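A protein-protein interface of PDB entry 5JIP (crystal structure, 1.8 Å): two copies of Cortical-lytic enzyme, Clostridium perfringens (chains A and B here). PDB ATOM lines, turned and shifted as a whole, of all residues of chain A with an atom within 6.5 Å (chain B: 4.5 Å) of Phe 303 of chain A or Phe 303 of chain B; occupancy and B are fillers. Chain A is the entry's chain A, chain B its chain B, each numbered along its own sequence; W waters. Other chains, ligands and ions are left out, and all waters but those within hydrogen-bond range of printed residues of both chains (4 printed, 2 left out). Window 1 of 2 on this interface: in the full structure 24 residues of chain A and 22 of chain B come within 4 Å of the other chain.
Of the printed residues of chain B, Phe 303 of chain A touches Phe 303 (3.99 Å).
Of the printed residues of chain A, Thr 273 of chain B touches Asn 263 and Phe 309.
Of the printed residues of chain A, Phe 303 of chain B touches Phe 303 (3.99 Å).
Printed residues of chain A within 4 Å of Phe 309 of chain B: Thr 273.
The nearest printed residue of chain B that does not touch Phe 303 of chain A is Thr 273 of chain B (4.3 Å).
Hydrophobic or aromatic side chains of chain A that line the printed part of chain B: Phe 303 and Phe 309.
Along chain A the printed residues that touch a printed residue of chain B span positions 260 to 309.
Of the 13 printed residues of chain B, 5 touch a printed residue of chain A.
Printed residues of chain B that touch a printed residue of chain A: Asn 260, Asn 263, Thr 273, Phe 303 and Phe 309.
Hydrophobic or aromatic side chains of chain B within 4 Å of the printed part of chain A: Phe 303 and Phe 309.
Among the printed residues, 6 pairs touch across the chains.
Among the printed residues, no Asp or Glu carboxylate lies within 4 Å of a Lys or Arg side-chain nitrogen of the other chain.
Asn 260 of chain B touches its own counterpart, Asn 260 of chain A.
Asn 263 of chain A touches Thr 273 of chain B, and with the chains exchanged Thr 273 of chain A touches Asn 263 of chain B.
Thr 273 of chain A touches Phe 309 of chain B, and with the chains exchanged Phe 309 of chain A touches Thr 273 of chain B.
Phe 303 of chain A touches its own counterpart, Phe 303 of chain B.
Positions printed for both chains: 232, 259, 260, 261, 262, 263, 273, 301, 302, 303, 304, 308 and 309.
Of the 6 pairs that touch across the chains among the printed residues, 6 have their exchanged pair printed and touching as well.
The side-chain amide oxygen (OD1) of Asn 260 of chain B is in hydrogen-bond range of the side-chain amide nitrogen (ND2) of Asn 260 of chain A, 2.5 Å away.
The side-chain hydroxyl of Thr 273 of chain B is in hydrogen-bond range of the side-chain amide nitrogen of Asn 263 of chain A, at 3.0 Å.
ND2 of Asn 263 of chain B is in hydrogen-bond range of OG1 of Thr 273 of chain A, at 3.1 Å.
Water W2 lies within hydrogen-bond range of the side-chain amide nitrogen of Asn 260 of chain B (2.5 Å), the backbone carbonyl oxygen of Asp 304 of chain B (3.1 Å) and the backbone carbonyl oxygen of Asn 260 of chain A (3.2 Å).
Water W4 lies within hydrogen-bond range of the backbone carbonyl oxygen of Thr 273 of chain B (2.6 Å) and the backbone carbonyl oxygen of Gly 307 of chain A (2.8 Å).
Water W3 bridges O of Ile 305 of chain A and O of Asn 260 of chain B.
Water W1 bridges the backbone carbonyl oxygen (O) of Asn 260 of chain A (2.7 Å) and the side-chain amide nitrogen (ND2) of Asn 260 of chain B (3.4 Å).
CZ of Phe 309 of chain B touches O of Thr 273 of chain A, 3.5 Å away.
CZ of Phe 303 of chain B touches CZ of Phe 303 of chain A, at 3.99 Å.
CZ of Phe 309 of chain A touches O of Thr 273 of chain B (3.4 Å).
O of Gly 261 of chain A is in hydrogen-bond range of N of Phe 303 of chain A (2.8 Å).
The side-chain hydroxyl of Thr 273 of chain A sits at hydrogen-bond distance from the side-chain amide oxygen of Asn 263 of chain A (2.7 Å).
The backbone NH (N) of Asn 263 of chain A sits at hydrogen-bond distance from the backbone carbonyl oxygen (O) of Glu 301 of chain A, 2.9 Å away.
O of Gly 261 of chain B is in hydrogen-bond range of N of Phe 303 of chain B (2.9 Å).
The side-chain amide oxygen (OD1) of Asn 263 of chain B sits at hydrogen-bond distance from the side-chain hydroxyl (OG1) of Thr 273 of chain B (2.7 Å).
N of Asn 263 of chain B is in hydrogen-bond range of O of Glu 301 of chain B, at 2.9 Å.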
ATOM      1  N   PRO A 232      14.973 -32.403   9.348  1.00  0.00           N
ATOM      2  CA  PRO A 232      13.884 -33.321   8.989  1.00  0.00           C
ATOM      3  C   PRO A 232      14.246 -34.150   7.774  1.00  0.00           C
ATOM      4  O   PRO A 232      15.113 -33.784   6.968  1.00  0.00           O
ATOM      5  CB  PRO A 232      12.705 -32.397   8.670  1.00  0.00           C
ATOM      6  CG  PRO A 232      13.225 -31.084   8.583  1.00  0.00           C
ATOM      7  CD  PRO A 232      14.639 -31.006   9.034  1.00  0.00           C
ATOM      8  N   ASN A 254       5.097 -35.021   7.163  1.00  0.00           N
ATOM      9  CA  ASN A 254       6.312 -35.408   7.869  1.00  0.00           C
ATOM     10  C   ASN A 254       5.976 -35.700   9.321  1.00  0.00           C
ATOM     11  O   ASN A 254       4.992 -35.207   9.857  1.00  0.00           O
ATOM     12  CB  ASN A 254       7.377 -34.313   7.805  1.00  0.00           C
ATOM     13  CG  ASN A 254       8.328 -34.475   6.651  1.00  0.00           C
ATOM     14  OD1 ASN A 254       7.933 -34.575   5.482  1.00  0.00           O
ATOM     15  ND2 ASN A 254       9.627 -34.483   6.975  1.00  0.00           N
ATOM     16  N   ASP A 258       9.833 -32.113  15.911  1.00  0.00           N
ATOM     17  CA  ASP A 258      10.179 -30.708  15.829  1.00  0.00           C
ATOM     18  C   ASP A 258       9.828 -30.113  14.473  1.00  0.00           C
ATOM     19  O   ASP A 258      10.376 -29.069  14.108  1.00  0.00           O
ATOM     20  CB  ASP A 258      11.677 -30.506  16.116  1.00  0.00           C
ATOM     21  CG  ASP A 258      12.562 -31.178  15.079  1.00  0.00           C
ATOM     22  OD1 ASP A 258      12.073 -32.100  14.360  1.00  0.00           O
ATOM     23  OD2 ASP A 258      13.765 -30.830  14.992  1.00  0.00           O
ATOM     24  N   LEU A 259       8.958 -30.780  13.705  1.00  0.00           N
ATOM     25  CA  LEU A 259       8.541 -30.260  12.416  1.00  0.00           C
ATOM     26  C   LEU A 259       7.914 -28.878  12.584  1.00  0.00           C
ATOM     27  O   LEU A 259       7.133 -28.626  13.507  1.00  0.00           O
ATOM     28  CB  LEU A 259       7.543 -31.207  11.776  1.00  0.00           C
ATOM     29  CG  LEU A 259       7.048 -30.817  10.396  1.00  0.00           C
ATOM     30  CD1 LEU A 259       8.144 -30.930   9.374  1.00  0.00           C
ATOM     31  CD2 LEU A 259       5.870 -31.692  10.070  1.00  0.00           C
ATOM     32  N   ASN A 260       8.271 -27.972  11.689  1.00  0.00           N
ATOM     33  CA  ASN A 260       7.738 -26.638  11.749  1.00  0.00           C
ATOM     34  C   ASN A 260       7.097 -26.146  10.465  1.00  0.00           C
ATOM     35  O   ASN A 260       6.363 -25.162  10.529  1.00  0.00           O
ATOM     36  CB  ASN A 260       8.824 -25.654  12.171  1.00  0.00           C
ATOM     37  CG  ASN A 260       8.299 -24.642  13.141  1.00  0.00           C
ATOM     38  OD1 ASN A 260       7.192 -24.800  13.655  1.00  0.00           O
ATOM     39  ND2 ASN A 260       9.074 -23.582  13.392  1.00  0.00           N
ATOM     40  N   GLY A 261       7.316 -26.794   9.325  1.00  0.00           N
ATOM     41  CA  GLY A 261       6.621 -26.406   8.114  1.00  0.00           C
ATOM     42  C   GLY A 261       7.324 -26.920   6.872  1.00  0.00           C
ATOM     43  O   GLY A 261       8.234 -27.738   6.942  1.00  0.00           O
ATOM     44  N   TYR A 262       6.891 -26.383   5.742  1.00  0.00           N
ATOM     45  CA  TYR A 262       7.350 -26.769   4.421  1.00  0.00           C
ATOM     46  C   TYR A 262       7.436 -25.536   3.547  1.00  0.00           C
ATOM     47  O   TYR A 262       6.633 -24.605   3.679  1.00  0.00           O
ATOM     48  CB  TYR A 262       6.403 -27.767   3.731  1.00  0.00           C
ATOM     49  CG  TYR A 262       5.957 -28.931   4.557  1.00  0.00           C
ATOM     50  CD1 TYR A 262       4.885 -28.812   5.432  1.00  0.00           C
ATOM     51  CD2 TYR A 262       6.566 -30.177   4.419  1.00  0.00           C
ATOM     52  CE1 TYR A 262       4.475 -29.879   6.195  1.00  0.00           C
ATOM     53  CE2 TYR A 262       6.162 -31.243   5.155  1.00  0.00           C
ATOM     54  CZ  TYR A 262       5.104 -31.115   6.025  1.00  0.00           C
ATOM     55  OH  TYR A 262       4.721 -32.211   6.746  1.00  0.00           O
ATOM     56  N   ASN A 263       8.400 -25.555   2.640  1.00  0.00           N
ATOM     57  CA  ASN A 263       8.459 -24.644   1.507  1.00  0.00           C
ATOM     58  C   ASN A 263       8.252 -25.443   0.226  1.00  0.00           C
ATOM     59  O   ASN A 263       8.856 -26.505   0.037  1.00  0.00           O
ATOM     60  CB  ASN A 263       9.803 -23.921   1.425  1.00  0.00           C
ATOM     61  CG  ASN A 263      10.018 -22.951   2.570  1.00  0.00           C
ATOM     62  OD1 ASN A 263       9.085 -22.271   3.022  1.00  0.00           O
ATOM     63  ND2 ASN A 263      11.239 -22.923   3.092  1.00  0.00           N
ATOM     64  N   THR A 273       4.992 -21.019   1.870  1.00  0.00           N
ATOM     65  CA  THR A 273       5.393 -21.663   3.113  1.00  0.00           C
ATOM     66  C   THR A 273       4.154 -22.171   3.829  1.00  0.00           C
ATOM     67  O   THR A 273       3.177 -21.435   3.976  1.00  0.00           O
ATOM     68  CB  THR A 273       6.173 -20.697   4.007  1.00  0.00           C
ATOM     69  OG1 THR A 273       7.317 -20.226   3.292  1.00  0.00           O
ATOM     70  CG2 THR A 273       6.623 -21.370   5.286  1.00  0.00           C
ATOM     71  N   LEU A 274       4.188 -23.433   4.245  1.00  0.00           N
ATOM     72  CA  LEU A 274       3.058 -24.049   4.939  1.00  0.00           C
ATOM     73  C   LEU A 274       3.456 -24.383   6.372  1.00  0.00           C
ATOM     74  O   LEU A 274       4.640 -24.618   6.646  1.00  0.00           O
ATOM     75  CB  LEU A 274       2.602 -25.331   4.240  1.00  0.00           C
ATOM     76  CG  LEU A 274       2.060 -25.272   2.811  1.00  0.00           C
ATOM     77  CD1 LEU A 274       0.963 -24.225   2.703  1.00  0.00           C
ATOM     78  CD2 LEU A 274       3.184 -25.055   1.830  1.00  0.00           C
ATOM     79  N   PRO A 275       2.505 -24.434   7.306  1.00  0.00           N
ATOM     80  CA  PRO A 275       2.820 -24.788   8.692  1.00  0.00           C
ATOM     81  C   PRO A 275       2.904 -26.309   8.865  1.00  0.00           C
ATOM     82  O   PRO A 275       2.642 -27.090   7.951  1.00  0.00           O
ATOM     83  CB  PRO A 275       1.650 -24.189   9.477  1.00  0.00           C
ATOM     84  CG  PRO A 275       0.470 -24.319   8.481  1.00  0.00           C
ATOM     85  CD  PRO A 275       1.092 -24.034   7.145  1.00  0.00           C
ATOM     86  N   GLU A 301      10.499 -28.942   0.544  1.00  0.00           N
ATOM     87  CA  GLU A 301      11.365 -29.239   1.673  1.00  0.00           C
ATOM     88  C   GLU A 301      10.591 -29.043   2.974  1.00  0.00           C
ATOM     89  O   GLU A 301       9.791 -28.109   3.108  1.00  0.00           O
ATOM     90  CB  GLU A 301      12.621 -28.345   1.658  1.00  0.00           C
ATOM     91  CG  GLU A 301      12.310 -26.839   1.845  1.00  0.00           C
ATOM     92  CD  GLU A 301      13.484 -25.934   1.520  1.00  0.00           C
ATOM     93  OE1 GLU A 301      14.522 -26.434   1.019  1.00  0.00           O
ATOM     94  OE2 GLU A 301      13.355 -24.693   1.755  1.00  0.00           O
ATOM     95  N   ALA A 302      10.829 -29.934   3.927  1.00  0.00           N
ATOM     96  CA  ALA A 302      10.404 -29.692   5.293  1.00  0.00           C
ATOM     97  C   ALA A 302      11.453 -28.854   6.017  1.00  0.00           C
ATOM     98  O   ALA A 302      12.621 -28.814   5.628  1.00  0.00           O
ATOM     99  CB  ALA A 302      10.181 -31.003   6.030  1.00  0.00           C
ATOM    100  N   PHE A 303      11.028 -28.163   7.080  1.00  0.00           N
ATOM    101  CA  PHE A 303      12.002 -27.529   7.967  1.00  0.00           C
ATOM    102  C   PHE A 303      11.510 -27.655   9.401  1.00  0.00           C
ATOM    103  O   PHE A 303      10.314 -27.846   9.650  1.00  0.00           O
ATOM    104  CB  PHE A 303      12.300 -26.049   7.604  1.00  0.00           C
ATOM    105  CG  PHE A 303      11.097 -25.129   7.570  1.00  0.00           C
ATOM    106  CD1 PHE A 303      10.633 -24.498   8.724  1.00  0.00           C
ATOM    107  CD2 PHE A 303      10.469 -24.848   6.366  1.00  0.00           C
ATOM    108  CE1 PHE A 303       9.538 -23.634   8.675  1.00  0.00           C
ATOM    109  CE2 PHE A 303       9.400 -23.979   6.305  1.00  0.00           C
ATOM    110  CZ  PHE A 303       8.917 -23.371   7.454  1.00  0.00           C
ATOM    111  N   ASP A 304      12.450 -27.590  10.345  1.00  0.00           N
ATOM    112  CA  ASP A 304      12.145 -27.845  11.746  1.00  0.00           C
ATOM    113  C   ASP A 304      12.274 -26.553  12.559  1.00  0.00           C
ATOM    114  O   ASP A 304      12.587 -25.489  12.033  1.00  0.00           O
ATOM    115  CB  ASP A 304      13.005 -28.995  12.289  1.00  0.00           C
ATOM    116  CG  ASP A 304      14.502 -28.700  12.296  1.00  0.00           C
ATOM    117  OD1 ASP A 304      14.916 -27.530  12.160  1.00  0.00           O
ATOM    118  OD2 ASP A 304      15.267 -29.676  12.456  1.00  0.00           O
ATOM    119  N   ILE A 305      11.960 -26.649  13.855  1.00  0.00           N
ATOM    120  CA  ILE A 305      11.821 -25.459  14.685  1.00  0.00           C
ATOM    121  C   ILE A 305      13.088 -24.630  14.715  1.00  0.00           C
ATOM    122  O   ILE A 305      13.023 -23.399  14.777  1.00  0.00           O
ATOM    123  CB  ILE A 305      11.372 -25.867  16.100  1.00  0.00           C
ATOM    124  CG1 ILE A 305       9.945 -26.404  16.003  1.00  0.00           C
ATOM    125  CG2 ILE A 305      11.434 -24.675  17.061  1.00  0.00           C
ATOM    126  CD1 ILE A 305       9.437 -27.031  17.316  1.00  0.00           C
ATOM    127  N   THR A 306      14.257 -25.260  14.666  1.00  0.00           N
ATOM    128  CA  THR A 306      15.489 -24.492  14.754  1.00  0.00           C
ATOM    129  C   THR A 306      16.070 -24.182  13.382  1.00  0.00           C
ATOM    130  O   THR A 306      17.167 -23.650  13.297  1.00  0.00           O
ATOM    131  CB  THR A 306      16.500 -25.199  15.676  1.00  0.00           C
ATOM    132  OG1 THR A 306      16.544 -26.601  15.408  1.00  0.00           O
ATOM    133  CG2 THR A 306      16.074 -25.017  17.133  1.00  0.00           C
ATOM    134  N   GLY A 307      15.333 -24.445  12.304  1.00  0.00           N
ATOM    135  CA  GLY A 307      15.683 -23.866  11.023  1.00  0.00           C
ATOM    136  C   GLY A 307      16.560 -24.700  10.119  1.00  0.00           C
ATOM    137  O   GLY A 307      17.200 -24.138   9.216  1.00  0.00           O
ATOM    138  N   ASP A 308      16.629 -26.018  10.328  1.00  0.00           N
ATOM    139  CA  ASP A 308      17.209 -26.924   9.354  1.00  0.00           C
ATOM    140  C   ASP A 308      16.154 -27.481   8.411  1.00  0.00           C
ATOM    141  O   ASP A 308      14.969 -27.604   8.751  1.00  0.00           O
ATOM    142  CB  ASP A 308      17.934 -28.080  10.042  1.00  0.00           C
ATOM    143  CG  ASP A 308      19.308 -27.678  10.572  1.00  0.00           C
ATOM    144  OD1 ASP A 308      20.092 -27.103   9.809  1.00  0.00           O
ATOM    145  OD2 ASP A 308      19.585 -27.909  11.765  1.00  0.00           O
ATOM    146  N   PHE A 309      16.614 -27.836   7.217  1.00  0.00           N
ATOM    147  CA  PHE A 309      15.777 -28.289   6.114  1.00  0.00           C
ATOM    148  C   PHE A 309      16.080 -29.727   5.718  1.00  0.00           C
ATOM    149  O   PHE A 309      17.175 -30.239   5.953  1.00  0.00           O
ATOM    150  CB  PHE A 309      15.989 -27.408   4.897  1.00  0.00           C
ATOM    151  CG  PHE A 309      15.838 -25.963   5.200  1.00  0.00           C
ATOM    152  CD1 PHE A 309      16.908 -25.237   5.681  1.00  0.00           C
ATOM    153  CD2 PHE A 309      14.621 -25.340   5.054  1.00  0.00           C
ATOM    154  CE1 PHE A 309      16.768 -23.882   5.978  1.00  0.00           C
ATOM    155  CE2 PHE A 309      14.479 -24.001   5.385  1.00  0.00           C
ATOM    156  CZ  PHE A 309      15.557 -23.284   5.849  1.00  0.00           C
ATOM    157  N   SER A 310      15.088 -30.350   5.086  1.00  0.00           N
ATOM    158  CA  SER A 310      15.284 -31.591   4.335  1.00  0.00           C
ATOM    159  C   SER A 310      16.552 -31.481   3.515  1.00  0.00           C
ATOM    160  O   SER A 310      16.754 -30.503   2.801  1.00  0.00           O
ATOM    161  CB  SER A 310      14.092 -31.861   3.397  1.00  0.00           C
ATOM    162  OG  SER A 310      12.856 -31.890   4.090  1.00  0.00           O
ATOM    163  N   PRO B 232       1.592 -12.211  12.515  1.00  0.00           N
ATOM    164  CA  PRO B 232       2.649 -11.378  13.097  1.00  0.00           C
ATOM    165  C   PRO B 232       2.691  -9.993  12.470  1.00  0.00           C
ATOM    166  O   PRO B 232       2.273  -9.767  11.330  1.00  0.00           O
ATOM    167  CB  PRO B 232       3.940 -12.141  12.799  1.00  0.00           C
ATOM    168  CG  PRO B 232       3.613 -13.254  11.955  1.00  0.00           C
ATOM    169  CD  PRO B 232       2.124 -13.308  11.699  1.00  0.00           C
ATOM    170  N   LEU B 259       5.695 -16.563  17.290  1.00  0.00           N
ATOM    171  CA  LEU B 259       6.628 -16.380  16.184  1.00  0.00           C
ATOM    172  C   LEU B 259       7.261 -17.698  15.812  1.00  0.00           C
ATOM    173  O   LEU B 259       7.655 -18.490  16.676  1.00  0.00           O
ATOM    174  CB  LEU B 259       7.722 -15.394  16.556  1.00  0.00           C
ATOM    175  CG  LEU B 259       8.727 -15.054  15.470  1.00  0.00           C
ATOM    176  CD1 LEU B 259       8.069 -14.392  14.239  1.00  0.00           C
ATOM    177  CD2 LEU B 259       9.770 -14.158  16.103  1.00  0.00           C
ATOM    178  N   ASN B 260       7.413 -17.909  14.518  1.00  0.00           N
ATOM    179  CA  ASN B 260       7.997 -19.143  14.054  1.00  0.00           C
ATOM    180  C   ASN B 260       9.135 -18.969  13.076  1.00  0.00           C
ATOM    181  O   ASN B 260       9.881 -19.923  12.890  1.00  0.00           O
ATOM    182  CB  ASN B 260       6.922 -20.019  13.415  1.00  0.00           C
ATOM    183  CG  ASN B 260       7.072 -21.467  13.795  1.00  0.00           C
ATOM    184  OD1 ASN B 260       7.852 -21.808  14.692  1.00  0.00           O
ATOM    185  ND2 ASN B 260       6.341 -22.338  13.103  1.00  0.00           N
ATOM    186  N   GLY B 261       9.308 -17.805  12.468  1.00  0.00           N
ATOM    187  CA  GLY B 261      10.432 -17.594  11.584  1.00  0.00           C
ATOM    188  C   GLY B 261      10.211 -16.443  10.626  1.00  0.00           C
ATOM    189  O   GLY B 261       9.285 -15.643  10.769  1.00  0.00           O
ATOM    190  N   TYR B 262      11.116 -16.373   9.657  1.00  0.00           N
ATOM    191  CA  TYR B 262      11.126 -15.315   8.661  1.00  0.00           C
ATOM    192  C   TYR B 262      11.468 -15.928   7.316  1.00  0.00           C
ATOM    193  O   TYR B 262      12.228 -16.891   7.236  1.00  0.00           O
ATOM    194  CB  TYR B 262      12.175 -14.232   8.974  1.00  0.00           C
ATOM    195  CG  TYR B 262      12.137 -13.682  10.378  1.00  0.00           C
ATOM    196  CD1 TYR B 262      12.773 -14.335  11.432  1.00  0.00           C
ATOM    197  CD2 TYR B 262      11.487 -12.484  10.649  1.00  0.00           C
ATOM    198  CE1 TYR B 262      12.723 -13.844  12.722  1.00  0.00           C
ATOM    199  CE2 TYR B 262      11.442 -11.965  11.945  1.00  0.00           C
ATOM    200  CZ  TYR B 262      12.080 -12.635  12.974  1.00  0.00           C
ATOM    201  OH  TYR B 262      12.048 -12.098  14.262  1.00  0.00           O
ATOM    202  N   ASN B 263      10.917 -15.353   6.259  1.00  0.00           N
ATOM    203  CA  ASN B 263      11.403 -15.547   4.902  1.00  0.00           C
ATOM    204  C   ASN B 263      12.008 -14.248   4.388  1.00  0.00           C
ATOM    205  O   ASN B 263      11.436 -13.175   4.571  1.00  0.00           O
ATOM    206  CB  ASN B 263      10.296 -15.976   3.955  1.00  0.00           C
ATOM    207  CG  ASN B 263       9.770 -17.373   4.254  1.00  0.00           C
ATOM    208  OD1 ASN B 263      10.529 -18.311   4.550  1.00  0.00           O
ATOM    209  ND2 ASN B 263       8.450 -17.512   4.191  1.00  0.00           N
ATOM    210  N   THR B 273      14.808 -19.131   4.648  1.00  0.00           N
ATOM    211  CA  THR B 273      13.925 -19.205   5.804  1.00  0.00           C
ATOM    212  C   THR B 273      14.776 -19.296   7.057  1.00  0.00           C
ATOM    213  O   THR B 273      15.717 -20.097   7.115  1.00  0.00           O
ATOM    214  CB  THR B 273      12.999 -20.424   5.738  1.00  0.00           C
ATOM    215  OG1 THR B 273      12.243 -20.436   4.529  1.00  0.00           O
ATOM    216  CG2 THR B 273      12.053 -20.503   6.944  1.00  0.00           C
ATOM    217  N   GLU B 301       9.500 -11.095   5.616  1.00  0.00           N
ATOM    218  CA  GLU B 301       8.256 -11.296   6.328  1.00  0.00           C
ATOM    219  C   GLU B 301       8.490 -12.242   7.498  1.00  0.00           C
ATOM    220  O   GLU B 301       9.252 -13.202   7.386  1.00  0.00           O
ATOM    221  CB  GLU B 301       7.162 -11.884   5.386  1.00  0.00           C
ATOM    222  CG  GLU B 301       7.528 -13.293   4.854  1.00  0.00           C
ATOM    223  CD  GLU B 301       6.629 -13.800   3.741  1.00  0.00           C
ATOM    224  OE1 GLU B 301       5.794 -13.024   3.209  1.00  0.00           O
ATOM    225  OE2 GLU B 301       6.758 -15.006   3.413  1.00  0.00           O
ATOM    226  N   ALA B 302       7.783 -11.997   8.598  1.00  0.00           N
ATOM    227  CA  ALA B 302       7.671 -12.950   9.681  1.00  0.00           C
ATOM    228  C   ALA B 302       6.508 -13.902   9.438  1.00  0.00           C
ATOM    229  O   ALA B 302       5.571 -13.566   8.721  1.00  0.00           O
ATOM    230  CB  ALA B 302       7.469 -12.197  10.989  1.00  0.00           C
ATOM    231  N   PHE B 303       6.582 -15.107  10.014  1.00  0.00           N
ATOM    232  CA  PHE B 303       5.411 -15.980  10.035  1.00  0.00           C
ATOM    233  C   PHE B 303       5.308 -16.660  11.395  1.00  0.00           C
ATOM    234  O   PHE B 303       6.280 -16.739  12.153  1.00  0.00           O
ATOM    235  CB  PHE B 303       5.401 -17.006   8.898  1.00  0.00           C
ATOM    236  CG  PHE B 303       6.610 -17.880   8.821  1.00  0.00           C
ATOM    237  CD1 PHE B 303       6.659 -19.090   9.476  1.00  0.00           C
ATOM    238  CD2 PHE B 303       7.673 -17.528   7.988  1.00  0.00           C
ATOM    239  CE1 PHE B 303       7.762 -19.919   9.353  1.00  0.00           C
ATOM    240  CE2 PHE B 303       8.761 -18.333   7.886  1.00  0.00           C
ATOM    241  CZ  PHE B 303       8.807 -19.533   8.556  1.00  0.00           C
ATOM    242  N   ASP B 304       4.080 -17.072  11.740  1.00  0.00           N
ATOM    243  CA  ASP B 304       3.831 -17.669  13.037  1.00  0.00           C
ATOM    244  C   ASP B 304       3.569 -19.165  12.901  1.00  0.00           C
ATOM    245  O   ASP B 304       3.581 -19.729  11.813  1.00  0.00           O
ATOM    246  CB  ASP B 304       2.691 -16.963  13.780  1.00  0.00           C
ATOM    247  CG  ASP B 304       1.359 -16.982  13.049  1.00  0.00           C
ATOM    248  OD1 ASP B 304       1.112 -17.890  12.213  1.00  0.00           O
ATOM    249  OD2 ASP B 304       0.539 -16.077  13.365  1.00  0.00           O
ATOM    250  N   ASP B 308       0.404 -17.928   9.377  1.00  0.00           N
ATOM    251  CA  ASP B 308       0.107 -16.589   8.886  1.00  0.00           C
ATOM    252  C   ASP B 308       1.382 -15.741   8.831  1.00  0.00           C
ATOM    253  O   ASP B 308       2.328 -15.946   9.593  1.00  0.00           O
ATOM    254  CB  ASP B 308      -0.927 -15.899   9.760  1.00  0.00           C
ATOM    255  CG  ASP B 308      -2.345 -16.329   9.433  1.00  0.00           C
ATOM    256  OD1 ASP B 308      -2.699 -16.285   8.242  1.00  0.00           O
ATOM    257  OD2 ASP B 308      -3.071 -16.720  10.363  1.00  0.00           O
ATOM    258  N   PHE B 309       1.374 -14.764   7.922  1.00  0.00           N
ATOM    259  CA  PHE B 309       2.527 -13.953   7.592  1.00  0.00           C
ATOM    260  C   PHE B 309       2.268 -12.498   7.974  1.00  0.00           C
ATOM    261  O   PHE B 309       1.124 -12.056   8.042  1.00  0.00           O
ATOM    262  CB  PHE B 309       2.843 -14.007   6.096  1.00  0.00           C
ATOM    263  CG  PHE B 309       3.045 -15.399   5.587  1.00  0.00           C
ATOM    264  CD1 PHE B 309       1.969 -16.127   5.115  1.00  0.00           C
ATOM    265  CD2 PHE B 309       4.288 -15.999   5.642  1.00  0.00           C
ATOM    266  CE1 PHE B 309       2.132 -17.431   4.671  1.00  0.00           C
ATOM    267  CE2 PHE B 309       4.467 -17.311   5.214  1.00  0.00           C
ATOM    268  CZ  PHE B 309       3.390 -18.019   4.704  1.00  0.00           C
HETATM  269  O   HOH W   1       4.267 -24.861  12.266  1.00  0.00           O
HETATM  270  O   HOH W   2       4.988 -22.344  10.996  1.00  0.00           O
HETATM  271  O   HOH W   3      11.318 -21.272  14.942  1.00  0.00           O
HETATM  272  O   HOH W   4      17.326 -21.400   8.756  1.00  0.00           O
